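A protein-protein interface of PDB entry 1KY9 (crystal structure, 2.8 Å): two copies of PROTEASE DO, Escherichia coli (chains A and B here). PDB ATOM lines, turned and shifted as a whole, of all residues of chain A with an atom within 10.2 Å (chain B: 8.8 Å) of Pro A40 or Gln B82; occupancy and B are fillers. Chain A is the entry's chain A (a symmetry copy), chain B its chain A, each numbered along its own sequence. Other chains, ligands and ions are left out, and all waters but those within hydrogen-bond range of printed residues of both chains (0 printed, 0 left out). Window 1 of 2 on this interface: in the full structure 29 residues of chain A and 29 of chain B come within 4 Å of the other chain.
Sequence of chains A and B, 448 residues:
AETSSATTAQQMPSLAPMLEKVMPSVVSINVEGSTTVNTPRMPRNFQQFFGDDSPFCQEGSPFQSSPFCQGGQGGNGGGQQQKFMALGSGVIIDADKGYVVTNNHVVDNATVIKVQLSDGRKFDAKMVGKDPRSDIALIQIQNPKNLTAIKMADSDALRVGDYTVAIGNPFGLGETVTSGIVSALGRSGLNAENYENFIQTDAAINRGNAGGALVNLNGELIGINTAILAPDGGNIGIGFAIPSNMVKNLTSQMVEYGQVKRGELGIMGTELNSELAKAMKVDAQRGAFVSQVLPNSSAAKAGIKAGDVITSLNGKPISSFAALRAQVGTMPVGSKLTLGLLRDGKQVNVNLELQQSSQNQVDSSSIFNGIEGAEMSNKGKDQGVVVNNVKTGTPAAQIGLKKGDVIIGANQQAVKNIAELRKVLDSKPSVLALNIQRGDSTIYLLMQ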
ATOM      1  N   THR A  35      -5.248  29.271 -18.905  1.00  0.00           N
ATOM      2  CA  THR A  35      -6.178  29.969 -19.782  1.00  0.00           C
ATOM      3  C   THR A  35      -6.849  29.007 -20.761  1.00  0.00           C
ATOM      4  O   THR A  35      -6.250  28.013 -21.156  1.00  0.00           O
ATOM      5  CB  THR A  35      -5.432  31.043 -20.580  1.00  0.00           C
ATOM      6  OG1 THR A  35      -6.267  31.506 -21.638  1.00  0.00           O
ATOM      7  CG2 THR A  35      -4.132  30.470 -21.168  1.00  0.00           C
ATOM      8  N   THR A  36      -8.086  29.297 -21.150  1.00  0.00           N
ATOM      9  CA  THR A  36      -8.800  28.450 -22.102  1.00  0.00           C
ATOM     10  C   THR A  36      -8.323  28.713 -23.532  1.00  0.00           C
ATOM     11  O   THR A  36      -8.389  29.845 -24.025  1.00  0.00           O
ATOM     12  CB  THR A  36     -10.322  28.683 -22.038  1.00  0.00           C
ATOM     13  OG1 THR A  36     -10.942  27.621 -21.296  1.00  0.00           O
ATOM     14  CG2 THR A  36     -10.914  28.756 -23.440  1.00  0.00           C
ATOM     15  N   VAL A  37      -7.855  27.656 -24.197  1.00  0.00           N
ATOM     16  CA  VAL A  37      -7.344  27.771 -25.564  1.00  0.00           C
ATOM     17  C   VAL A  37      -7.953  26.756 -26.545  1.00  0.00           C
ATOM     18  O   VAL A  37      -8.494  25.718 -26.141  1.00  0.00           O
ATOM     19  CB  VAL A  37      -5.809  27.610 -25.584  1.00  0.00           C
ATOM     20  CG1 VAL A  37      -5.444  26.167 -25.361  1.00  0.00           C
ATOM     21  CG2 VAL A  37      -5.249  28.109 -26.894  1.00  0.00           C
ATOM     22  N   ASN A  38      -7.864  27.092 -27.834  1.00  0.00           N
ATOM     23  CA  ASN A  38      -8.359  26.247 -28.927  1.00  0.00           C
ATOM     24  C   ASN A  38      -7.497  24.981 -29.079  1.00  0.00           C
ATOM     25  O   ASN A  38      -6.270  25.050 -28.968  1.00  0.00           O
ATOM     26  CB  ASN A  38      -8.305  27.014 -30.257  1.00  0.00           C
ATOM     27  CG  ASN A  38      -9.585  27.789 -30.559  1.00  0.00           C
ATOM     28  OD1 ASN A  38     -10.691  27.241 -30.514  1.00  0.00           O
ATOM     29  ND2 ASN A  38      -9.435  29.068 -30.896  1.00  0.00           N
ATOM     30  N   THR A  39      -8.130  23.835 -29.332  1.00  0.00           N
ATOM     31  CA  THR A  39      -7.382  22.596 -29.527  1.00  0.00           C
ATOM     32  C   THR A  39      -6.701  22.667 -30.901  1.00  0.00           C
ATOM     33  O   THR A  39      -7.362  22.789 -31.933  1.00  0.00           O
ATOM     34  CB  THR A  39      -8.303  21.346 -29.517  1.00  0.00           C
ATOM     35  OG1 THR A  39      -8.964  21.219 -28.248  1.00  0.00           O
ATOM     36  CG2 THR A  39      -7.481  20.091 -29.785  1.00  0.00           C
ATOM     37  N   PRO A  40      -5.364  22.604 -30.931  1.00  0.00           N
ATOM     38  CA  PRO A  40      -4.646  22.665 -32.199  1.00  0.00           C
ATOM     39  C   PRO A  40      -5.204  21.708 -33.244  1.00  0.00           C
ATOM     40  O   PRO A  40      -5.437  20.537 -32.957  1.00  0.00           O
ATOM     41  CB  PRO A  40      -3.227  22.284 -31.800  1.00  0.00           C
ATOM     42  CG  PRO A  40      -3.114  22.829 -30.466  1.00  0.00           C
ATOM     43  CD  PRO A  40      -4.422  22.486 -29.811  1.00  0.00           C
ATOM     44  N   ARG A  41      -5.413  22.217 -34.455  1.00  0.00           N
ATOM     45  CA  ARG A  41      -5.897  21.408 -35.575  1.00  0.00           C
ATOM     46  C   ARG A  41      -4.701  21.075 -36.479  1.00  0.00           C
ATOM     47  O   ARG A  41      -3.949  21.961 -36.905  1.00  0.00           O
ATOM     48  CB  ARG A  41      -6.970  22.167 -36.358  1.00  0.00           C
ATOM     49  CG  ARG A  41      -7.233  21.622 -37.757  1.00  0.00           C
ATOM     50  CD  ARG A  41      -6.271  22.199 -38.822  1.00  0.00           C
ATOM     51  NE  ARG A  41      -6.549  21.674 -40.164  1.00  0.00           N
ATOM     52  CZ  ARG A  41      -5.873  22.003 -41.266  1.00  0.00           C
ATOM     53  NH1 ARG A  41      -4.865  22.867 -41.209  1.00  0.00           N
ATOM     54  NH2 ARG A  41      -6.210  21.463 -42.431  1.00  0.00           N
ATOM     55  N   MET A  42      -4.518  19.795 -36.773  1.00  0.00           N
ATOM     56  CA  MET A  42      -3.393  19.390 -37.600  1.00  0.00           C
ATOM     57  C   MET A  42      -3.671  18.296 -38.634  1.00  0.00           C
ATOM     58  O   MET A  42      -4.762  17.712 -38.673  1.00  0.00           O
ATOM     59  CB  MET A  42      -2.241  19.002 -36.685  1.00  0.00           C
ATOM     60  CG  MET A  42      -1.804  20.182 -35.827  1.00  0.00           C
ATOM     61  SD  MET A  42      -0.327  19.781 -34.697  1.00  0.00           S
ATOM     62  CE  MET A  42      -0.209  17.867 -35.034  1.00  0.00           C
ATOM     63  N   PRO A  43      -2.680  18.000 -39.492  1.00  0.00           N
ATOM     64  CA  PRO A  43      -1.325  18.572 -39.603  1.00  0.00           C
ATOM     65  C   PRO A  43      -1.298  20.088 -39.831  1.00  0.00           C
ATOM     66  O   PRO A  43      -2.238  20.664 -40.389  1.00  0.00           O
ATOM     67  CB  PRO A  43      -0.725  17.830 -40.797  1.00  0.00           C
ATOM     68  CG  PRO A  43      -1.722  16.722 -41.101  1.00  0.00           C
ATOM     69  CD  PRO A  43      -3.027  17.266 -40.716  1.00  0.00           C
ATOM     70  N   ARG A  44      -0.215  20.733 -39.405  1.00  0.00           N
ATOM     71  CA  ARG A  44      -0.089  22.170 -39.601  1.00  0.00           C
ATOM     72  C   ARG A  44       0.419  22.447 -41.004  1.00  0.00           C
ATOM     73  O   ARG A  44       1.534  22.057 -41.325  1.00  0.00           O
ATOM     74  CB  ARG A  44       0.892  22.785 -38.592  1.00  0.00           C
ATOM     75  CG  ARG A  44       0.262  23.142 -37.250  1.00  0.00           C
ATOM     76  CD  ARG A  44       1.027  24.258 -36.514  1.00  0.00           C
ATOM     77  NE  ARG A  44       2.147  23.778 -35.703  1.00  0.00           N
ATOM     78  CZ  ARG A  44       2.939  24.566 -34.976  1.00  0.00           C
ATOM     79  NH1 ARG A  44       2.742  25.880 -34.957  1.00  0.00           N
ATOM     80  NH2 ARG A  44       3.926  24.043 -34.256  1.00  0.00           N
ATOM     81  N   ASN A  45      -0.394  23.101 -41.835  1.00  0.00           N
ATOM     82  CA  ASN A  45       0.019  23.457 -43.199  1.00  0.00           C
ATOM     83  C   ASN A  45       0.292  24.964 -43.240  1.00  0.00           C
ATOM     84  O   ASN A  45      -0.637  25.773 -43.194  1.00  0.00           O
ATOM     85  CB  ASN A  45      -1.066  23.096 -44.225  1.00  0.00           C
ATOM     86  CG  ASN A  45      -0.590  23.268 -45.665  1.00  0.00           C
ATOM     87  OD1 ASN A  45       0.408  23.937 -45.930  1.00  0.00           O
ATOM     88  ND2 ASN A  45      -1.313  22.667 -46.599  1.00  0.00           N
ATOM     89  N   PHE A  50      -6.251  29.189 -41.511  1.00  0.00           N
ATOM     90  CA  PHE A  50      -7.255  28.418 -40.774  1.00  0.00           C
ATOM     91  C   PHE A  50      -7.875  29.148 -39.573  1.00  0.00           C
ATOM     92  O   PHE A  50      -7.181  29.847 -38.826  1.00  0.00           O
ATOM     93  CB  PHE A  50      -6.636  27.087 -40.311  1.00  0.00           C
ATOM     94  CG  PHE A  50      -7.628  26.125 -39.691  1.00  0.00           C
ATOM     95  CD1 PHE A  50      -8.732  25.672 -40.418  1.00  0.00           C
ATOM     96  CD2 PHE A  50      -7.455  25.667 -38.383  1.00  0.00           C
ATOM     97  CE1 PHE A  50      -9.650  24.782 -39.853  1.00  0.00           C
ATOM     98  CE2 PHE A  50      -8.366  24.777 -37.809  1.00  0.00           C
ATOM     99  CZ  PHE A  50      -9.467  24.334 -38.547  1.00  0.00           C
ATOM    100  N   GLY A  79     -11.723  23.105 -27.233  1.00  0.00           N
ATOM    101  CA  GLY A  79     -11.185  23.997 -26.219  1.00  0.00           C
ATOM    102  C   GLY A  79     -10.595  23.250 -25.034  1.00  0.00           C
ATOM    103  O   GLY A  79     -11.201  22.311 -24.522  1.00  0.00           O
ATOM    104  N   GLN A  80      -9.410  23.678 -24.599  1.00  0.00           N
ATOM    105  CA  GLN A  80      -8.703  23.060 -23.477  1.00  0.00           C
ATOM    106  C   GLN A  80      -8.000  24.125 -22.624  1.00  0.00           C
ATOM    107  O   GLN A  80      -7.816  25.262 -23.060  1.00  0.00           O
ATOM    108  CB  GLN A  80      -7.671  22.075 -24.018  1.00  0.00           C
ATOM    109  CG  GLN A  80      -6.933  22.617 -25.229  1.00  0.00           C
ATOM    110  CD  GLN A  80      -5.750  21.765 -25.641  1.00  0.00           C
ATOM    111  OE1 GLN A  80      -5.059  22.071 -26.618  1.00  0.00           O
ATOM    112  NE2 GLN A  80      -5.502  20.693 -24.896  1.00  0.00           N
ATOM    113  N   GLN A  81      -7.620  23.754 -21.403  1.00  0.00           N
ATOM    114  CA  GLN A  81      -6.928  24.671 -20.505  1.00  0.00           C
ATOM    115  C   GLN A  81      -5.436  24.605 -20.751  1.00  0.00           C
ATOM    116  O   GLN A  81      -4.871  23.514 -20.838  1.00  0.00           O
ATOM    117  CB  GLN A  81      -7.174  24.308 -19.033  1.00  0.00           C
ATOM    118  CG  GLN A  81      -8.434  24.881 -18.404  1.00  0.00           C
ATOM    119  CD  GLN A  81      -8.829  26.245 -18.975  1.00  0.00           C
ATOM    120  OE1 GLN A  81      -9.506  26.324 -20.009  1.00  0.00           O
ATOM    121  NE2 GLN A  81      -8.399  27.319 -18.311  1.00  0.00           N
ATOM    122  N   GLN A  82      -4.788  25.762 -20.852  1.00  0.00           N
ATOM    123  CA  GLN A  82      -3.343  25.786 -21.045  1.00  0.00           C
ATOM    124  C   GLN A  82      -2.659  26.627 -19.968  1.00  0.00           C
ATOM    125  O   GLN A  82      -3.072  27.761 -19.705  1.00  0.00           O
ATOM    126  CB  GLN A  82      -2.987  26.323 -22.440  1.00  0.00           C
ATOM    127  CG  GLN A  82      -1.476  26.335 -22.703  1.00  0.00           C
ATOM    128  CD  GLN A  82      -1.107  26.546 -24.173  1.00  0.00           C
ATOM    129  OE1 GLN A  82      -1.452  27.563 -24.786  1.00  0.00           O
ATOM    130  NE2 GLN A  82      -0.391  25.577 -24.739  1.00  0.00           N
ATOM    131  N   LYS A  83      -1.631  26.063 -19.337  1.00  0.00           N
ATOM    132  CA  LYS A  83      -0.876  26.769 -18.300  1.00  0.00           C
ATOM    133  C   LYS A  83       0.088  27.767 -18.910  1.00  0.00           C
ATOM    134  O   LYS A  83       0.728  27.473 -19.898  1.00  0.00           O
ATOM    135  CB  LYS A  83      -0.069  25.800 -17.446  1.00  0.00           C
ATOM    136  CG  LYS A  83      -0.854  25.232 -16.298  1.00  0.00           C
ATOM    137  CD  LYS A  83       0.038  24.495 -15.312  1.00  0.00           C
ATOM    138  CE  LYS A  83      -0.698  24.301 -13.984  1.00  0.00           C
ATOM    139  NZ  LYS A  83      -1.062  25.632 -13.363  1.00  0.00           N
ATOM    140  N   PHE A  84       0.194  28.950 -18.327  1.00  0.00           N
ATOM    141  CA  PHE A  84       1.099  29.945 -18.857  1.00  0.00           C
ATOM    142  C   PHE A  84       1.901  30.516 -17.707  1.00  0.00           C
ATOM    143  O   PHE A  84       1.595  30.272 -16.553  1.00  0.00           O
ATOM    144  CB  PHE A  84       0.314  31.055 -19.567  1.00  0.00           C
ATOM    145  CG  PHE A  84      -0.440  31.957 -18.643  1.00  0.00           C
ATOM    146  CD1 PHE A  84       0.197  33.020 -18.008  1.00  0.00           C
ATOM    147  CD2 PHE A  84      -1.790  31.753 -18.399  1.00  0.00           C
ATOM    148  CE1 PHE A  84      -0.500  33.874 -17.139  1.00  0.00           C
ATOM    149  CE2 PHE A  84      -2.506  32.601 -17.533  1.00  0.00           C
ATOM    150  CZ  PHE A  84      -1.857  33.663 -16.902  1.00  0.00           C
ATOM    151  N   VAL B  31      -8.221  11.759 -35.602  1.00  0.00           N
ATOM    152  CA  VAL B  31      -7.252  11.495 -34.561  1.00  0.00           C
ATOM    153  C   VAL B  31      -7.352  12.473 -33.408  1.00  0.00           C
ATOM    154  O   VAL B  31      -7.521  13.664 -33.608  1.00  0.00           O
ATOM    155  CB  VAL B  31      -5.818  11.593 -35.137  1.00  0.00           C
ATOM    156  CG1 VAL B  31      -4.810  11.711 -34.036  1.00  0.00           C
ATOM    157  CG2 VAL B  31      -5.525  10.392 -35.967  1.00  0.00           C
ATOM    158  N   GLU B  32      -7.251  11.956 -32.196  1.00  0.00           N
ATOM    159  CA  GLU B  32      -7.248  12.803 -31.027  1.00  0.00           C
ATOM    160  C   GLU B  32      -5.985  12.394 -30.307  1.00  0.00           C
ATOM    161  O   GLU B  32      -5.806  11.232 -29.940  1.00  0.00           O
ATOM    162  CB  GLU B  32      -8.462  12.542 -30.167  1.00  0.00           C
ATOM    163  CG  GLU B  32      -8.619  13.547 -29.055  1.00  0.00           C
ATOM    164  CD  GLU B  32      -9.911  13.368 -28.256  1.00  0.00           C
ATOM    165  OE1 GLU B  32      -9.897  13.784 -27.071  1.00  0.00           O
ATOM    166  OE2 GLU B  32     -10.918  12.835 -28.802  1.00  0.00           O
ATOM    167  N   GLY B  33      -5.072  13.338 -30.157  1.00  0.00           N
ATOM    168  CA  GLY B  33      -3.830  13.022 -29.480  1.00  0.00           C
ATOM    169  C   GLY B  33      -3.299  14.122 -28.578  1.00  0.00           C
ATOM    170  O   GLY B  33      -3.748  15.261 -28.617  1.00  0.00           O
ATOM    171  N   SER B  34      -2.320  13.769 -27.767  1.00  0.00           N
ATOM    172  CA  SER B  34      -1.722  14.717 -26.861  1.00  0.00           C
ATOM    173  C   SER B  34      -0.243  14.845 -27.149  1.00  0.00           C
ATOM    174  O   SER B  34       0.398  13.897 -27.536  1.00  0.00           O
ATOM    175  CB  SER B  34      -1.924  14.251 -25.441  1.00  0.00           C
ATOM    176  OG  SER B  34      -1.019  14.928 -24.606  1.00  0.00           O
ATOM    177  N   THR B  35       0.314  16.023 -26.946  1.00  0.00           N
ATOM    178  CA  THR B  35       1.731  16.226 -27.214  1.00  0.00           C
ATOM    179  C   THR B  35       2.373  17.134 -26.167  1.00  0.00           C
ATOM    180  O   THR B  35       1.712  18.012 -25.626  1.00  0.00           O
ATOM    181  CB  THR B  35       1.911  16.864 -28.595  1.00  0.00           C
ATOM    182  OG1 THR B  35       3.250  17.333 -28.724  1.00  0.00           O
ATOM    183  CG2 THR B  35       0.938  18.039 -28.776  1.00  0.00           C
ATOM    184  N   THR B  36       3.653  16.923 -25.880  1.00  0.00           N
ATOM    185  CA  THR B  36       4.360  17.755 -24.908  1.00  0.00           C
ATOM    186  C   THR B  36       4.752  19.099 -25.525  1.00  0.00           C
ATOM    187  O   THR B  36       5.458  19.151 -26.538  1.00  0.00           O
ATOM    188  CB  THR B  36       5.631  17.061 -24.385  1.00  0.00           C
ATOM    189  OG1 THR B  36       5.381  16.516 -23.079  1.00  0.00           O
ATOM    190  CG2 THR B  36       6.795  18.044 -24.326  1.00  0.00           C
ATOM    191  N   VAL B  37       4.300  20.187 -24.897  1.00  0.00           N
ATOM    192  CA  VAL B  37       4.581  21.535 -25.393  1.00  0.00           C
ATOM    193  C   VAL B  37       5.154  22.484 -24.329  1.00  0.00           C
ATOM    194  O   VAL B  37       5.010  22.255 -23.120  1.00  0.00           O
ATOM    195  CB  VAL B  37       3.304  22.173 -25.981  1.00  0.00           C
ATOM    196  CG1 VAL B  37       2.371  22.565 -24.868  1.00  0.00           C
ATOM    197  CG2 VAL B  37       3.661  23.368 -26.829  1.00  0.00           C
ATOM    198  N   ASN B  38       5.818  23.539 -24.810  1.00  0.00           N
ATOM    199  CA  ASN B  38       6.416  24.576 -23.960  1.00  0.00           C
ATOM    200  C   ASN B  38       5.329  25.424 -23.279  1.00  0.00           C
ATOM    201  O   ASN B  38       4.321  25.762 -23.907  1.00  0.00           O
ATOM    202  CB  ASN B  38       7.287  25.515 -24.806  1.00  0.00           C
ATOM    203  CG  ASN B  38       8.740  25.061 -24.913  1.00  0.00           C
ATOM    204  OD1 ASN B  38       9.400  24.783 -23.904  1.00  0.00           O
ATOM    205  ND2 ASN B  38       9.255  25.010 -26.138  1.00  0.00           N
ATOM    206  N   PRO B  40       3.618  28.581 -22.419  1.00  0.00           N
ATOM    207  CA  PRO B  40       3.666  29.937 -22.954  1.00  0.00           C
ATOM    208  C   PRO B  40       4.251  30.943 -21.972  1.00  0.00           C
ATOM    209  O   PRO B  40       3.866  30.973 -20.806  1.00  0.00           O
ATOM    210  CB  PRO B  40       2.203  30.235 -23.248  1.00  0.00           C
ATOM    211  CG  PRO B  40       1.684  28.940 -23.628  1.00  0.00           C
ATOM    212  CD  PRO B  40       2.292  27.989 -22.635  1.00  0.00           C
ATOM    213  N   GLY B  79       7.136  22.831 -19.433  1.00  0.00           N
ATOM    214  CA  GLY B  79       6.558  21.864 -20.353  1.00  0.00           C
ATOM    215  C   GLY B  79       5.248  21.283 -19.845  1.00  0.00           C
ATOM    216  O   GLY B  79       5.142  20.904 -18.681  1.00  0.00           O
ATOM    217  N   GLN B  80       4.255  21.207 -20.730  1.00  0.00           N
ATOM    218  CA  GLN B  80       2.930  20.685 -20.399  1.00  0.00           C
ATOM    219  C   GLN B  80       2.360  19.865 -21.566  1.00  0.00           C
ATOM    220  O   GLN B  80       2.842  19.959 -22.696  1.00  0.00           O
ATOM    221  CB  GLN B  80       1.995  21.848 -20.087  1.00  0.00           C
ATOM    222  CG  GLN B  80       2.178  23.011 -21.046  1.00  0.00           C
ATOM    223  CD  GLN B  80       1.113  24.077 -20.908  1.00  0.00           C
ATOM    224  OE1 GLN B  80       1.136  25.091 -21.612  1.00  0.00           O
ATOM    225  NE2 GLN B  80       0.164  23.855 -20.003  1.00  0.00           N
ATOM    226  N   GLN B  81       1.342  19.056 -21.284  1.00  0.00           N
ATOM    227  CA  GLN B  81       0.704  18.240 -22.311  1.00  0.00           C
ATOM    228  C   GLN B  81      -0.396  19.031 -22.987  1.00  0.00           C
ATOM    229  O   GLN B  81      -1.211  19.658 -22.311  1.00  0.00           O
ATOM    230  CB  GLN B  81       0.070  16.977 -21.711  1.00  0.00           C
ATOM    231  CG  GLN B  81       0.993  15.779 -21.546  1.00  0.00           C
ATOM    232  CD  GLN B  81       2.084  15.704 -22.615  1.00  0.00           C
ATOM    233  OE1 GLN B  81       3.143  16.331 -22.481  1.00  0.00           O
ATOM    234  NE2 GLN B  81       1.825  14.947 -23.683  1.00  0.00           N
ATOM    235  N   GLN B  82      -0.436  18.997 -24.316  1.00  0.00           N
ATOM    236  CA  GLN B  82      -1.490  19.695 -25.042  1.00  0.00           C
ATOM    237  C   GLN B  82      -2.234  18.743 -25.980  1.00  0.00           C
ATOM    238  O   GLN B  82      -1.607  18.005 -26.745  1.00  0.00           O
ATOM    239  CB  GLN B  82      -0.916  20.877 -25.837  1.00  0.00           C
ATOM    240  CG  GLN B  82      -1.994  21.665 -26.591  1.00  0.00           C
ATOM    241  CD  GLN B  82      -1.515  23.020 -27.115  1.00  0.00           C
ATOM    242  OE1 GLN B  82      -0.572  23.109 -27.910  1.00  0.00           O
ATOM    243  NE2 GLN B  82      -2.180  24.085 -26.672  1.00  0.00           N
ATOM    244  N   LYS B  83      -3.564  18.750 -25.901  1.00  0.00           N
ATOM    245  CA  LYS B  83      -4.395  17.903 -26.759  1.00  0.00           C
ATOM    246  C   LYS B  83      -4.506  18.482 -28.155  1.00  0.00           C
ATOM    247  O   LYS B  83      -4.659  19.675 -28.313  1.00  0.00           O
ATOM    248  CB  LYS B  83      -5.803  17.761 -26.197  1.00  0.00           C
ATOM    249  CG  LYS B  83      -5.930  16.644 -25.200  1.00  0.00           C
ATOM    250  CD  LYS B  83      -7.382  16.345 -24.866  1.00  0.00           C
ATOM    251  CE  LYS B  83      -7.494  14.972 -24.199  1.00  0.00           C
ATOM    252  NZ  LYS B  83      -7.004  13.877 -25.121  1.00  0.00           N
ATOM    253  N   PHE B  84      -4.427  17.640 -29.174  1.00  0.00           N
ATOM    254  CA  PHE B  84      -4.530  18.127 -30.531  1.00  0.00           C
ATOM    255  C   PHE B  84      -5.502  17.242 -31.279  1.00  0.00           C
ATOM    256  O   PHE B  84      -5.894  16.195 -30.791  1.00  0.00           O
ATOM    257  CB  PHE B  84      -3.154  18.108 -31.210  1.00  0.00           C
ATOM    258  CG  PHE B  84      -2.653  16.738 -31.537  1.00  0.00           C
ATOM    259  CD1 PHE B  84      -3.069  16.087 -32.695  1.00  0.00           C
ATOM    260  CD2 PHE B  84      -1.767  16.088 -30.693  1.00  0.00           C
ATOM    261  CE1 PHE B  84      -2.605  14.799 -33.015  1.00  0.00           C
ATOM    262  CE2 PHE B  84      -1.289  14.799 -30.997  1.00  0.00           C
ATOM    263  CZ  PHE B  84      -1.711  14.154 -32.162  1.00  0.00           C
ATOM    264  N   MET B  85      -5.902  17.675 -32.461  1.00  0.00           N
ATOM    265  CA  MET B  85      -6.794  16.885 -33.274  1.00  0.00           C
ATOM    266  C   MET B  85      -6.247  16.864 -34.681  1.00  0.00           C
ATOM    267  O   MET B  85      -6.179  17.897 -35.310  1.00  0.00           O
ATOM    268  CB  MET B  85      -8.181  17.491 -33.280  1.00  0.00           C
ATOM    269  CG  MET B  85      -9.000  17.164 -32.048  1.00  0.00           C
ATOM    270  SD  MET B  85     -10.787  17.918 -32.206  1.00  0.00           S
ATOM    271  CE  MET B  85     -11.451  16.828 -33.681  1.00  0.00           C
ATOM    272  N   ALA B  86      -5.828  15.701 -35.167  1.00  0.00           N
ATOM    273  CA  ALA B  86      -5.323  15.592 -36.532  1.00  0.00           C
ATOM    274  C   ALA B  86      -6.423  14.966 -37.351  1.00  0.00           C
ATOM    275  O   ALA B  86      -7.344  14.358 -36.828  1.00  0.00           O
ATOM    276  CB  ALA B  86      -4.093  14.737 -36.593  1.00  0.00           C
ATOM    277  N   LEU B  87      -6.328  15.089 -38.650  1.00  0.00           N
ATOM    278  CA  LEU B  87      -7.382  14.548 -39.482  1.00  0.00           C
ATOM    279  C   LEU B  87      -6.776  14.140 -40.814  1.00  0.00           C
ATOM    280  O   LEU B  87      -5.789  14.731 -41.252  1.00  0.00           O
ATOM    281  CB  LEU B  87      -8.447  15.625 -39.612  1.00  0.00           C
ATOM    282  CG  LEU B  87      -9.560  15.563 -40.613  1.00  0.00           C
ATOM    283  CD1 LEU B  87     -10.465  16.760 -40.426  1.00  0.00           C
ATOM    284  CD2 LEU B  87      -8.953  15.569 -41.997  1.00  0.00           C
ATOM    285  N   ASN B 109       1.443  10.271 -32.502  1.00  0.00           N
ATOM    286  CA  ASN B 109       1.040  10.769 -31.187  1.00  0.00           C
ATOM    287  C   ASN B 109      -0.442  10.690 -30.917  1.00  0.00           C
ATOM    288  O   ASN B 109      -0.974  11.455 -30.118  1.00  0.00           O
ATOM    289  CB  ASN B 109       1.461  12.217 -31.013  1.00  0.00           C
ATOM    290  CG  ASN B 109       2.932  12.360 -30.984  1.00  0.00           C
ATOM    291  OD1 ASN B 109       3.603  11.660 -30.218  1.00  0.00           O
ATOM    292  ND2 ASN B 109       3.469  13.248 -31.830  1.00  0.00           N
ATOM    293  N   THR B 111      -3.928   9.127 -29.522  1.00  0.00           N
ATOM    294  CA  THR B 111      -4.336   8.489 -28.291  1.00  0.00           C
ATOM    295  C   THR B 111      -5.652   7.786 -28.573  1.00  0.00           C
ATOM    296  O   THR B 111      -5.999   6.776 -27.975  1.00  0.00           O
ATOM    297  CB  THR B 111      -4.552   9.540 -27.232  1.00  0.00           C
ATOM    298  OG1 THR B 111      -3.283   9.958 -26.739  1.00  0.00           O
ATOM    299  CG2 THR B 111      -5.371   9.010 -26.107  1.00  0.00           C
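Among the printed residues, merely in contact across the chains: Thr A39 with Lys B83 (3.2 Å), Thr A39 with Phe B84 (3.6 Å), Thr A39 with Met B85 (3.9 Å), Pro A40 with Gln B82 (3.6 Å), Pro A40 with Lys B83 (3.2 Å), Pro A40 with Phe B84 (3.5 Å), Arg A41 with Met B85 (3.5 Å), Met A42 with Ala B86 (3.1 Å), Pro A43 with Leu B87 (3.8 Å), Gln A80 with Gln B82 (3.1 Å), Gln A82 with Pro B40 (3.6 Å), Gln A82 with Gln B80 (3.1 Å), Lys A83 with Pro B40 (3.2 Å) and Phe A84 with Pro B40 (3.5 Å).
The side-chain amide nitrogen of Gln B82 lies close to the side-chain amide nitrogen of Gln A82 (3.0 Å). NE2 of Gln B80 sits close to N of Lys A83, at 2.9 Å. O of Met B85 lies within hydrogen-bond range of N of Met A42, 2.9 Å away. The backbone NH (N) of Lys B83 lies close to the side-chain amide nitrogen (NE2) of Gln A80, at 2.9 Å. The backbone carbonyl oxygen (O) of Pro A40 lies within hydrogen-bond range of the backbone NH (N) of Met B85 (2.9 Å). The backbone NH of Leu B87 is in hydrogen-bond range of the backbone carbonyl oxygen of Met A42 (3.1 Å).
Pro A40 touches just these residues of chain B: Gln B82, Lys B83, Phe B84 and Met B85. No residue of chain A comes within 4 Å of Ser B34. No residue of chain A comes within 4 Å of Thr B35. No residue of chain A comes within 4 Å of Gln B81. Of chain A, only Pro A40, Gln A80 and Gln A82 come within 4 Å of Gln B82. Printed residues of chain A within 4 Å of Phe B84: Thr A39 (3.6 Å) and Pro A40 (3.5 Å). Of the printed residues of chain A, Ala B86 touches Met A42. The nearest residue of chain B that does not touch Pro A40 is Ala B86 (5.3 Å). The nearest printed residue of chain A that does not touch Met B85 is Pro A43 (5.5 Å).
Of the 20 printed residues of chain B, 8 touch a printed residue of chain A. Among the printed residues, no Asp or Glu carboxylate lies within 4 Å of a Lys or Arg side-chain nitrogen of the other chain.
Pro A40 touches Gln B82, and with the chains exchanged Gln A82 touches Pro B40. Pro A40 touches Lys B83, and with the chains exchanged Lys A83 touches Pro B40. Gln A80 touches Lys B83, and with the chains exchanged Lys A83 touches Gln B80. Gln B82 touches its own counterpart, Gln A82. Of the 20 pairs that touch across the chains among the printed residues, 11 have their exchanged pair printed and touching as well.
The backbone carbonyl oxygen (O) of Gly B33 lies within hydrogen-bond range of the backbone NH (N) of Phe B84 (2.5 Å). The side-chain carboxylate (OE1) of Glu B32 lies within salt-bridge range of the side-chain amino group (NZ) of Lys B83 (3.5 Å). The backbone NH (N) of Val A37 sits at hydrogen-bond distance from the backbone carbonyl oxygen (O) of Gln A80, at 2.7 Å. The backbone carbonyl oxygen of Thr B35 lies within hydrogen-bond range of the backbone NH of Gln B82 (2.7 Å). O of Ala B86 lies within hydrogen-bond range of N of Val B31. The backbone carbonyl oxygen (O) of Thr A35 is in hydrogen-bond range of the backbone NH (N) of Gln A82.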
